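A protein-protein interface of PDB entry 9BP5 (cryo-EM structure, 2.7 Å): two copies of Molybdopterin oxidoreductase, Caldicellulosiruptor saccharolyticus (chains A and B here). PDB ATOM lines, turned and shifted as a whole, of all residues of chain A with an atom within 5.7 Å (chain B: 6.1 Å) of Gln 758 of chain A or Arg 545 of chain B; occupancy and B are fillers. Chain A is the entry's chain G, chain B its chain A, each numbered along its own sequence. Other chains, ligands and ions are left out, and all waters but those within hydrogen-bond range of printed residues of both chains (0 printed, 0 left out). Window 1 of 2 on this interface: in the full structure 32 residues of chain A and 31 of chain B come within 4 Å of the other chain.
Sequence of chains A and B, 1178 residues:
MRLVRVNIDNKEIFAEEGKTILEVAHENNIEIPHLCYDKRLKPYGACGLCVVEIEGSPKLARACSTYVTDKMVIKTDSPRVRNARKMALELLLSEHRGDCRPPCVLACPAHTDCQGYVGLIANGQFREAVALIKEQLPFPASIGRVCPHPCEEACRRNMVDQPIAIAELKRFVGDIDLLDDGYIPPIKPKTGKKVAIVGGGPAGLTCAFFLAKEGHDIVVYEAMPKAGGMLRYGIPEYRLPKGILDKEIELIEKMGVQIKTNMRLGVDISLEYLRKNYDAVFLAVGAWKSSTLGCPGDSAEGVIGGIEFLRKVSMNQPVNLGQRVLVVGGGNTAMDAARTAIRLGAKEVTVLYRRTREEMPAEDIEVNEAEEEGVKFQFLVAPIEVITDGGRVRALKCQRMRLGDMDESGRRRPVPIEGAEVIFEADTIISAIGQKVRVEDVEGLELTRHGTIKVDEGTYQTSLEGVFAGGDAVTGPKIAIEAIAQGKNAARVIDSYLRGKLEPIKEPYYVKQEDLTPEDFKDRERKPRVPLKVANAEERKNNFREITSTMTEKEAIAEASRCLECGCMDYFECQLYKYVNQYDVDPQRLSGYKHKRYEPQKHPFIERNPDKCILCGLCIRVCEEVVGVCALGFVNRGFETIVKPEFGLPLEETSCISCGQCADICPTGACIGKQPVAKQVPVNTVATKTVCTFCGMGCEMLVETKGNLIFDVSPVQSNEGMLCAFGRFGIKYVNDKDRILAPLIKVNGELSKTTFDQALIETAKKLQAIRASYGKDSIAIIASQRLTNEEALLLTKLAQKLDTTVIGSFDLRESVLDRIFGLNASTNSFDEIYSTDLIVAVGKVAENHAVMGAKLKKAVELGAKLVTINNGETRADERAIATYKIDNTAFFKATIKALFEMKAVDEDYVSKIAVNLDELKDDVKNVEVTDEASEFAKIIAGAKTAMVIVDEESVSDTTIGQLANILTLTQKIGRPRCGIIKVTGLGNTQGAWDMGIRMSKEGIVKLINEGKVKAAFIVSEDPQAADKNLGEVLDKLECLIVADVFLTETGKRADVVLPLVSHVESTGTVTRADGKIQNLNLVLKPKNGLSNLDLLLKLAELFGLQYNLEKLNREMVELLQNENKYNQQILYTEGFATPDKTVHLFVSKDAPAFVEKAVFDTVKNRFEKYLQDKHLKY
The guanidinium group (NH2) of Arg 545 of chain B is in hydrogen-bond range of the backbone carbonyl oxygen (O) of Lys 746 of chain A, 3.1 Å away.
The guanidinium group (NH2) of Arg 545 of chain B lies within salt-bridge range of the side-chain carboxylate (OE2) of Glu 762 of chain A (2.7 Å).
The side-chain amide oxygen of Asn 543 of chain B sits close to the backbone NH of Arg 545 of chain B.
N of Gln 758 of chain A is in hydrogen-bond range of OG1 of Thr 755 of chain A.
The side-chain amino group of Lys 766 of chain A is in salt-bridge range of the side-chain carboxylate of Glu 762 of chain A, at 3.3 Å.
Among the printed residues, merely in contact across the chains: Ile 745 of chain A with Arg 545 of chain B (3.9 Å), Lys 746 of chain A with Glu 539 of chain B (3.8 Å), Val 747 of chain A with Glu 539 of chain B (3.7 Å), Val 747 of chain A with Arg 545 of chain B (3.8 Å) and Gln 758 of chain A with Arg 545 of chain B (3.7 Å).
Printed residues of chain B within 4 Å of Lys 746 of chain A: Glu 539 and Arg 545.
Of the printed residues of chain B, Gln 758 of chain A touches Arg 545.
Of the printed residues of chain B, Glu 762 of chain A touches Arg 545.
Printed residues of chain A within 4 Å of Glu 539 of chain B: Lys 746 (3.8 Å) and Val 747 (3.7 Å).
Arg 545 of chain B touches five residues of chain A.
Of the 14 printed residues of chain A, 5 touch a printed residue of chain B.
No position is printed for both chains.
Of the 7 pairs that touch across the chains among the printed residues, none has its exchanged pair printed and touching as well.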
ATOM      1  N   ILE A 745      -2.922 -28.275  10.024  1.00  0.00           N
ATOM      2  CA  ILE A 745      -3.432 -29.447  10.723  1.00  0.00           C
ATOM      3  C   ILE A 745      -4.141 -30.331   9.712  1.00  0.00           C
ATOM      4  O   ILE A 745      -4.611 -29.860   8.675  1.00  0.00           O
ATOM      5  CB  ILE A 745      -4.377 -29.085  11.891  1.00  0.00           C
ATOM      6  CG1 ILE A 745      -5.474 -28.128  11.423  1.00  0.00           C
ATOM      7  CG2 ILE A 745      -3.595 -28.496  13.052  1.00  0.00           C
ATOM      8  CD1 ILE A 745      -6.560 -27.913  12.444  1.00  0.00           C
ATOM      9  N   LYS A 746      -4.214 -31.621  10.013  1.00  0.00           N
ATOM     10  CA  LYS A 746      -4.741 -32.602   9.073  1.00  0.00           C
ATOM     11  C   LYS A 746      -6.258 -32.655   9.194  1.00  0.00           C
ATOM     12  O   LYS A 746      -6.794 -33.188  10.168  1.00  0.00           O
ATOM     13  CB  LYS A 746      -4.124 -33.975   9.318  1.00  0.00           C
ATOM     14  CG  LYS A 746      -3.101 -34.372   8.278  1.00  0.00           C
ATOM     15  CD  LYS A 746      -3.006 -35.875   8.129  1.00  0.00           C
ATOM     16  CE  LYS A 746      -2.518 -36.525   9.407  1.00  0.00           C
ATOM     17  NZ  LYS A 746      -1.723 -37.749   9.123  1.00  0.00           N
ATOM     18  N   VAL A 747      -6.949 -32.105   8.199  1.00  0.00           N
ATOM     19  CA  VAL A 747      -8.392 -32.240   8.068  1.00  0.00           C
ATOM     20  C   VAL A 747      -8.665 -33.077   6.827  1.00  0.00           C
ATOM     21  O   VAL A 747      -7.991 -32.928   5.800  1.00  0.00           O
ATOM     22  CB  VAL A 747      -9.104 -30.872   8.006  1.00  0.00           C
ATOM     23  CG1 VAL A 747      -8.590 -29.961   9.108  1.00  0.00           C
ATOM     24  CG2 VAL A 747      -8.938 -30.213   6.653  1.00  0.00           C
ATOM     25  N   THR A 754      -4.617 -23.296   9.308  1.00  0.00           N
ATOM     26  CA  THR A 754      -5.447 -23.045  10.477  1.00  0.00           C
ATOM     27  C   THR A 754      -4.836 -21.885  11.258  1.00  0.00           C
ATOM     28  O   THR A 754      -3.914 -21.216  10.786  1.00  0.00           O
ATOM     29  CB  THR A 754      -5.586 -24.315  11.327  1.00  0.00           C
ATOM     30  OG1 THR A 754      -6.549 -24.094  12.363  1.00  0.00           O
ATOM     31  CG2 THR A 754      -4.259 -24.695  11.950  1.00  0.00           C
ATOM     32  N   THR A 755      -5.364 -21.637  12.451  1.00  0.00           N
ATOM     33  CA  THR A 755      -4.874 -20.583  13.324  1.00  0.00           C
ATOM     34  C   THR A 755      -3.885 -21.147  14.336  1.00  0.00           C
ATOM     35  O   THR A 755      -3.810 -22.355  14.562  1.00  0.00           O
ATOM     36  CB  THR A 755      -6.033 -19.895  14.049  1.00  0.00           C
ATOM     37  OG1 THR A 755      -6.416 -20.672  15.188  1.00  0.00           O
ATOM     38  CG2 THR A 755      -7.225 -19.758  13.124  1.00  0.00           C
ATOM     39  N   PHE A 756      -3.110 -20.245  14.942  1.00  0.00           N
ATOM     40  CA  PHE A 756      -2.083 -20.668  15.887  1.00  0.00           C
ATOM     41  C   PHE A 756      -2.692 -21.305  17.127  1.00  0.00           C
ATOM     42  O   PHE A 756      -2.178 -22.308  17.633  1.00  0.00           O
ATOM     43  CB  PHE A 756      -1.204 -19.482  16.275  1.00  0.00           C
ATOM     44  CG  PHE A 756      -0.034 -19.277  15.367  1.00  0.00           C
ATOM     45  CD1 PHE A 756       1.062 -20.114  15.430  1.00  0.00           C
ATOM     46  CD2 PHE A 756      -0.031 -18.250  14.444  1.00  0.00           C
ATOM     47  CE1 PHE A 756       2.139 -19.928  14.594  1.00  0.00           C
ATOM     48  CE2 PHE A 756       1.045 -18.061  13.605  1.00  0.00           C
ATOM     49  CZ  PHE A 756       2.131 -18.901  13.682  1.00  0.00           C
ATOM     50  N   ASP A 757      -3.784 -20.734  17.636  1.00  0.00           N
ATOM     51  CA  ASP A 757      -4.416 -21.277  18.833  1.00  0.00           C
ATOM     52  C   ASP A 757      -4.939 -22.685  18.590  1.00  0.00           C
ATOM     53  O   ASP A 757      -4.715 -23.593  19.400  1.00  0.00           O
ATOM     54  CB  ASP A 757      -5.544 -20.353  19.286  1.00  0.00           C
ATOM     55  CG  ASP A 757      -5.201 -18.891  19.108  1.00  0.00           C
ATOM     56  OD1 ASP A 757      -5.091 -18.440  17.948  1.00  0.00           O
ATOM     57  OD2 ASP A 757      -5.045 -18.189  20.128  1.00  0.00           O
ATOM     58  N   GLN A 758      -5.636 -22.887  17.471  1.00  0.00           N
ATOM     59  CA  GLN A 758      -6.174 -24.205  17.163  1.00  0.00           C
ATOM     60  C   GLN A 758      -5.060 -25.226  16.977  1.00  0.00           C
ATOM     61  O   GLN A 758      -5.151 -26.354  17.475  1.00  0.00           O
ATOM     62  CB  GLN A 758      -7.053 -24.129  15.915  1.00  0.00           C
ATOM     63  CG  GLN A 758      -7.670 -25.454  15.506  1.00  0.00           C
ATOM     64  CD  GLN A 758      -9.042 -25.669  16.114  1.00  0.00           C
ATOM     65  OE1 GLN A 758      -9.298 -25.279  17.252  1.00  0.00           O
ATOM     66  NE2 GLN A 758      -9.934 -26.295  15.354  1.00  0.00           N
ATOM     67  N   ALA A 759      -3.994 -24.843  16.272  1.00  0.00           N
ATOM     68  CA  ALA A 759      -2.888 -25.764  16.039  1.00  0.00           C
ATOM     69  C   ALA A 759      -2.176 -26.125  17.334  1.00  0.00           C
ATOM     70  O   ALA A 759      -1.810 -27.285  17.541  1.00  0.00           O
ATOM     71  CB  ALA A 759      -1.905 -25.157  15.045  1.00  0.00           C
ATOM     72  N   LEU A 760      -1.959 -25.145  18.212  1.00  0.00           N
ATOM     73  CA  LEU A 760      -1.295 -25.431  19.478  1.00  0.00           C
ATOM     74  C   LEU A 760      -2.160 -26.304  20.377  1.00  0.00           C
ATOM     75  O   LEU A 760      -1.648 -27.203  21.055  1.00  0.00           O
ATOM     76  CB  LEU A 760      -0.927 -24.130  20.180  1.00  0.00           C
ATOM     77  CG  LEU A 760       0.189 -23.337  19.506  1.00  0.00           C
ATOM     78  CD1 LEU A 760       0.331 -21.994  20.165  1.00  0.00           C
ATOM     79  CD2 LEU A 760       1.500 -24.096  19.544  1.00  0.00           C
ATOM     80  N   ILE A 761      -3.471 -26.055  20.401  1.00  0.00           N
ATOM     81  CA  ILE A 761      -4.369 -26.901  21.180  1.00  0.00           C
ATOM     82  C   ILE A 761      -4.351 -28.324  20.639  1.00  0.00           C
ATOM     83  O   ILE A 761      -4.326 -29.298  21.404  1.00  0.00           O
ATOM     84  CB  ILE A 761      -5.789 -26.306  21.183  1.00  0.00           C
ATOM     85  CG1 ILE A 761      -5.901 -25.209  22.235  1.00  0.00           C
ATOM     86  CG2 ILE A 761      -6.828 -27.377  21.455  1.00  0.00           C
ATOM     87  CD1 ILE A 761      -6.961 -24.192  21.928  1.00  0.00           C
ATOM     88  N   GLU A 762      -4.346 -28.467  19.313  1.00  0.00           N
ATOM     89  CA  GLU A 762      -4.273 -29.790  18.707  1.00  0.00           C
ATOM     90  C   GLU A 762      -2.969 -30.489  19.063  1.00  0.00           C
ATOM     91  O   GLU A 762      -2.963 -31.688  19.359  1.00  0.00           O
ATOM     92  CB  GLU A 762      -4.425 -29.674  17.193  1.00  0.00           C
ATOM     93  CG  GLU A 762      -4.389 -30.998  16.471  1.00  0.00           C
ATOM     94  CD  GLU A 762      -5.648 -31.258  15.682  1.00  0.00           C
ATOM     95  OE1 GLU A 762      -6.591 -30.448  15.791  1.00  0.00           O
ATOM     96  OE2 GLU A 762      -5.699 -32.271  14.955  1.00  0.00           O
ATOM     97  N   THR A 763      -1.855 -29.757  19.034  1.00  0.00           N
ATOM     98  CA  THR A 763      -0.564 -30.332  19.400  1.00  0.00           C
ATOM     99  C   THR A 763      -0.570 -30.820  20.841  1.00  0.00           C
ATOM    100  O   THR A 763      -0.139 -31.943  21.135  1.00  0.00           O
ATOM    101  CB  THR A 763       0.539 -29.293  19.200  1.00  0.00           C
ATOM    102  OG1 THR A 763       0.602 -28.913  17.823  1.00  0.00           O
ATOM    103  CG2 THR A 763       1.881 -29.842  19.631  1.00  0.00           C
ATOM    104  N   LYS A 766      -2.745 -33.934  21.174  1.00  0.00           N
ATOM    105  CA  LYS A 766      -2.129 -35.117  20.578  1.00  0.00           C
ATOM    106  C   LYS A 766      -1.027 -35.673  21.472  1.00  0.00           C
ATOM    107  O   LYS A 766      -0.955 -36.885  21.718  1.00  0.00           O
ATOM    108  CB  LYS A 766      -1.575 -34.777  19.195  1.00  0.00           C
ATOM    109  CG  LYS A 766      -2.637 -34.570  18.140  1.00  0.00           C
ATOM    110  CD  LYS A 766      -2.283 -35.278  16.855  1.00  0.00           C
ATOM    111  CE  LYS A 766      -3.403 -35.160  15.841  1.00  0.00           C
ATOM    112  NZ  LYS A 766      -4.726 -35.009  16.502  1.00  0.00           N
ATOM    113  N   GLU B 237     -13.232 -29.533  25.647  1.00  0.00           N
ATOM    114  CA  GLU B 237     -12.980 -28.491  24.656  1.00  0.00           C
ATOM    115  C   GLU B 237     -13.786 -28.705  23.380  1.00  0.00           C
ATOM    116  O   GLU B 237     -14.178 -27.731  22.727  1.00  0.00           O
ATOM    117  CB  GLU B 237     -11.482 -28.432  24.347  1.00  0.00           C
ATOM    118  CG  GLU B 237     -11.116 -27.696  23.067  1.00  0.00           C
ATOM    119  CD  GLU B 237     -10.688 -26.263  23.315  1.00  0.00           C
ATOM    120  OE1 GLU B 237     -10.301 -25.944  24.458  1.00  0.00           O
ATOM    121  OE2 GLU B 237     -10.737 -25.455  22.364  1.00  0.00           O
ATOM    122  N   TYR B 238     -14.064 -29.958  23.015  1.00  0.00           N
ATOM    123  CA  TYR B 238     -14.804 -30.204  21.782  1.00  0.00           C
ATOM    124  C   TYR B 238     -16.271 -29.814  21.886  1.00  0.00           C
ATOM    125  O   TYR B 238     -16.948 -29.741  20.856  1.00  0.00           O
ATOM    126  CB  TYR B 238     -14.688 -31.674  21.363  1.00  0.00           C
ATOM    127  CG  TYR B 238     -15.066 -32.675  22.427  1.00  0.00           C
ATOM    128  CD1 TYR B 238     -16.393 -33.015  22.649  1.00  0.00           C
ATOM    129  CD2 TYR B 238     -14.094 -33.303  23.188  1.00  0.00           C
ATOM    130  CE1 TYR B 238     -16.741 -33.933  23.614  1.00  0.00           C
ATOM    131  CE2 TYR B 238     -14.432 -34.231  24.150  1.00  0.00           C
ATOM    132  CZ  TYR B 238     -15.757 -34.538  24.362  1.00  0.00           C
ATOM    133  OH  TYR B 238     -16.098 -35.454  25.324  1.00  0.00           O
ATOM    134  N   ARG B 239     -16.776 -29.565  23.092  1.00  0.00           N
ATOM    135  CA  ARG B 239     -18.135 -29.076  23.274  1.00  0.00           C
ATOM    136  C   ARG B 239     -18.189 -27.596  23.614  1.00  0.00           C
ATOM    137  O   ARG B 239     -19.159 -26.923  23.254  1.00  0.00           O
ATOM    138  CB  ARG B 239     -18.840 -29.872  24.374  1.00  0.00           C
ATOM    139  CG  ARG B 239     -19.150 -31.305  23.989  1.00  0.00           C
ATOM    140  CD  ARG B 239     -19.898 -32.014  25.095  1.00  0.00           C
ATOM    141  NE  ARG B 239     -21.082 -31.261  25.488  1.00  0.00           N
ATOM    142  CZ  ARG B 239     -21.368 -30.911  26.733  1.00  0.00           C
ATOM    143  NH1 ARG B 239     -20.580 -31.241  27.742  1.00  0.00           N
ATOM    144  NH2 ARG B 239     -22.472 -30.210  26.970  1.00  0.00           N
ATOM    145  N   ARG B 343     -11.074 -40.024  22.880  1.00  0.00           N
ATOM    146  CA  ARG B 343     -10.194 -39.094  22.185  1.00  0.00           C
ATOM    147  C   ARG B 343      -8.762 -39.144  22.699  1.00  0.00           C
ATOM    148  O   ARG B 343      -7.855 -38.672  22.007  1.00  0.00           O
ATOM    149  CB  ARG B 343     -10.736 -37.672  22.304  1.00  0.00           C
ATOM    150  CG  ARG B 343     -11.792 -37.339  21.285  1.00  0.00           C
ATOM    151  CD  ARG B 343     -12.698 -36.240  21.775  1.00  0.00           C
ATOM    152  NE  ARG B 343     -13.690 -35.883  20.768  1.00  0.00           N
ATOM    153  CZ  ARG B 343     -14.866 -36.475  20.638  1.00  0.00           C
ATOM    154  NH1 ARG B 343     -15.243 -37.446  21.448  1.00  0.00           N
ATOM    155  NH2 ARG B 343     -15.687 -36.078  19.673  1.00  0.00           N
ATOM    156  N   GLU B 539     -13.683 -38.788  12.002  1.00  0.00           N
ATOM    157  CA  GLU B 539     -12.651 -37.769  12.134  1.00  0.00           C
ATOM    158  C   GLU B 539     -12.708 -37.091  13.498  1.00  0.00           C
ATOM    159  O   GLU B 539     -11.666 -36.772  14.079  1.00  0.00           O
ATOM    160  CB  GLU B 539     -12.784 -36.739  11.013  1.00  0.00           C
ATOM    161  CG  GLU B 539     -11.880 -35.522  11.168  1.00  0.00           C
ATOM    162  CD  GLU B 539     -11.311 -35.039   9.845  1.00  0.00           C
ATOM    163  OE1 GLU B 539     -12.099 -34.599   8.982  1.00  0.00           O
ATOM    164  OE2 GLU B 539     -10.075 -35.097   9.671  1.00  0.00           O
ATOM    165  N   ARG B 540     -13.912 -36.872  14.028  1.00  0.00           N
ATOM    166  CA  ARG B 540     -14.042 -36.116  15.266  1.00  0.00           C
ATOM    167  C   ARG B 540     -13.616 -36.911  16.489  1.00  0.00           C
ATOM    168  O   ARG B 540     -13.228 -36.305  17.492  1.00  0.00           O
ATOM    169  CB  ARG B 540     -15.480 -35.624  15.439  1.00  0.00           C
ATOM    170  CG  ARG B 540     -16.429 -36.644  16.019  1.00  0.00           C
ATOM    171  CD  ARG B 540     -17.803 -36.053  16.213  1.00  0.00           C
ATOM    172  NE  ARG B 540     -18.715 -37.011  16.821  1.00  0.00           N
ATOM    173  CZ  ARG B 540     -19.868 -37.383  16.289  1.00  0.00           C
ATOM    174  NH1 ARG B 540     -20.291 -36.885  15.141  1.00  0.00           N
ATOM    175  NH2 ARG B 540     -20.617 -38.277  16.925  1.00  0.00           N
ATOM    176  N   ASN B 543      -9.845 -36.129  17.612  1.00  0.00           N
ATOM    177  CA  ASN B 543      -9.381 -34.794  17.956  1.00  0.00           C
ATOM    178  C   ASN B 543     -10.355 -34.147  18.930  1.00  0.00           C
ATOM    179  O   ASN B 543     -11.430 -34.675  19.213  1.00  0.00           O
ATOM    180  CB  ASN B 543      -9.204 -33.915  16.710  1.00  0.00           C
ATOM    181  CG  ASN B 543     -10.396 -33.969  15.780  1.00  0.00           C
ATOM    182  OD1 ASN B 543     -11.308 -33.155  15.877  1.00  0.00           O
ATOM    183  ND2 ASN B 543     -10.390 -34.927  14.866  1.00  0.00           N
ATOM    184  N   PHE B 544      -9.950 -32.989  19.448  1.00  0.00           N
ATOM    185  CA  PHE B 544     -10.742 -32.211  20.391  1.00  0.00           C
ATOM    186  C   PHE B 544     -11.317 -30.956  19.746  1.00  0.00           C
ATOM    187  O   PHE B 544     -11.476 -29.930  20.407  1.00  0.00           O
ATOM    188  CB  PHE B 544      -9.906 -31.836  21.611  1.00  0.00           C
ATOM    189  CG  PHE B 544      -9.643 -32.981  22.541  1.00  0.00           C
ATOM    190  CD1 PHE B 544      -8.741 -33.973  22.204  1.00  0.00           C
ATOM    191  CD2 PHE B 544     -10.294 -33.062  23.758  1.00  0.00           C
ATOM    192  CE1 PHE B 544      -8.500 -35.022  23.058  1.00  0.00           C
ATOM    193  CE2 PHE B 544     -10.054 -34.114  24.614  1.00  0.00           C
ATOM    194  CZ  PHE B 544      -9.157 -35.093  24.262  1.00  0.00           C
ATOM    195  N   ARG B 545     -11.614 -31.017  18.453  1.00  0.00           N
ATOM    196  CA  ARG B 545     -12.196 -29.880  17.764  1.00  0.00           C
ATOM    197  C   ARG B 545     -13.693 -29.811  18.028  1.00  0.00           C
ATOM    198  O   ARG B 545     -14.338 -30.809  18.356  1.00  0.00           O
ATOM    199  CB  ARG B 545     -11.935 -29.967  16.263  1.00  0.00           C
ATOM    200  CG  ARG B 545     -10.472 -29.967  15.887  1.00  0.00           C
ATOM    201  CD  ARG B 545     -10.291 -30.144  14.393  1.00  0.00           C
ATOM    202  NE  ARG B 545      -8.937 -30.563  14.060  1.00  0.00           N
ATOM    203  CZ  ARG B 545      -8.628 -31.375  13.062  1.00  0.00           C
ATOM    204  NH1 ARG B 545      -9.557 -31.870  12.262  1.00  0.00           N
ATOM    205  NH2 ARG B 545      -7.356 -31.702  12.861  1.00  0.00           N
ATOM    206  N   GLU B 546     -14.244 -28.609  17.876  1.00  0.00           N
ATOM    207  CA  GLU B 546     -15.673 -28.410  18.070  1.00  0.00           C
ATOM    208  C   GLU B 546     -16.468 -29.306  17.133  1.00  0.00           C
ATOM    209  O   GLU B 546     -16.144 -29.447  15.953  1.00  0.00           O
ATOM    210  CB  GLU B 546     -16.037 -26.948  17.832  1.00  0.00           C
ATOM    211  CG  GLU B 546     -16.990 -26.371  18.855  1.00  0.00           C
ATOM    212  CD  GLU B 546     -17.370 -24.941  18.546  1.00  0.00           C
ATOM    213  OE1 GLU B 546     -16.580 -24.248  17.873  1.00  0.00           O
ATOM    214  OE2 GLU B 546     -18.458 -24.508  18.978  1.00  0.00           O
ATOM    215  N   ILE B 547     -17.520 -29.918  17.671  1.00  0.00           N
ATOM    216  CA  ILE B 547     -18.301 -30.873  16.896  1.00  0.00           C
ATOM    217  C   ILE B 547     -19.312 -30.162  16.011  1.00  0.00           C
ATOM    218  O   ILE B 547     -19.460 -30.494  14.832  1.00  0.00           O
ATOM    219  CB  ILE B 547     -18.980 -31.877  17.840  1.00  0.00           C
ATOM    220  CG1 ILE B 547     -17.922 -32.644  18.627  1.00  0.00           C
ATOM    221  CG2 ILE B 547     -19.864 -32.826  17.062  1.00  0.00           C
ATOM    222  CD1 ILE B 547     -18.488 -33.593  19.620  1.00  0.00           C
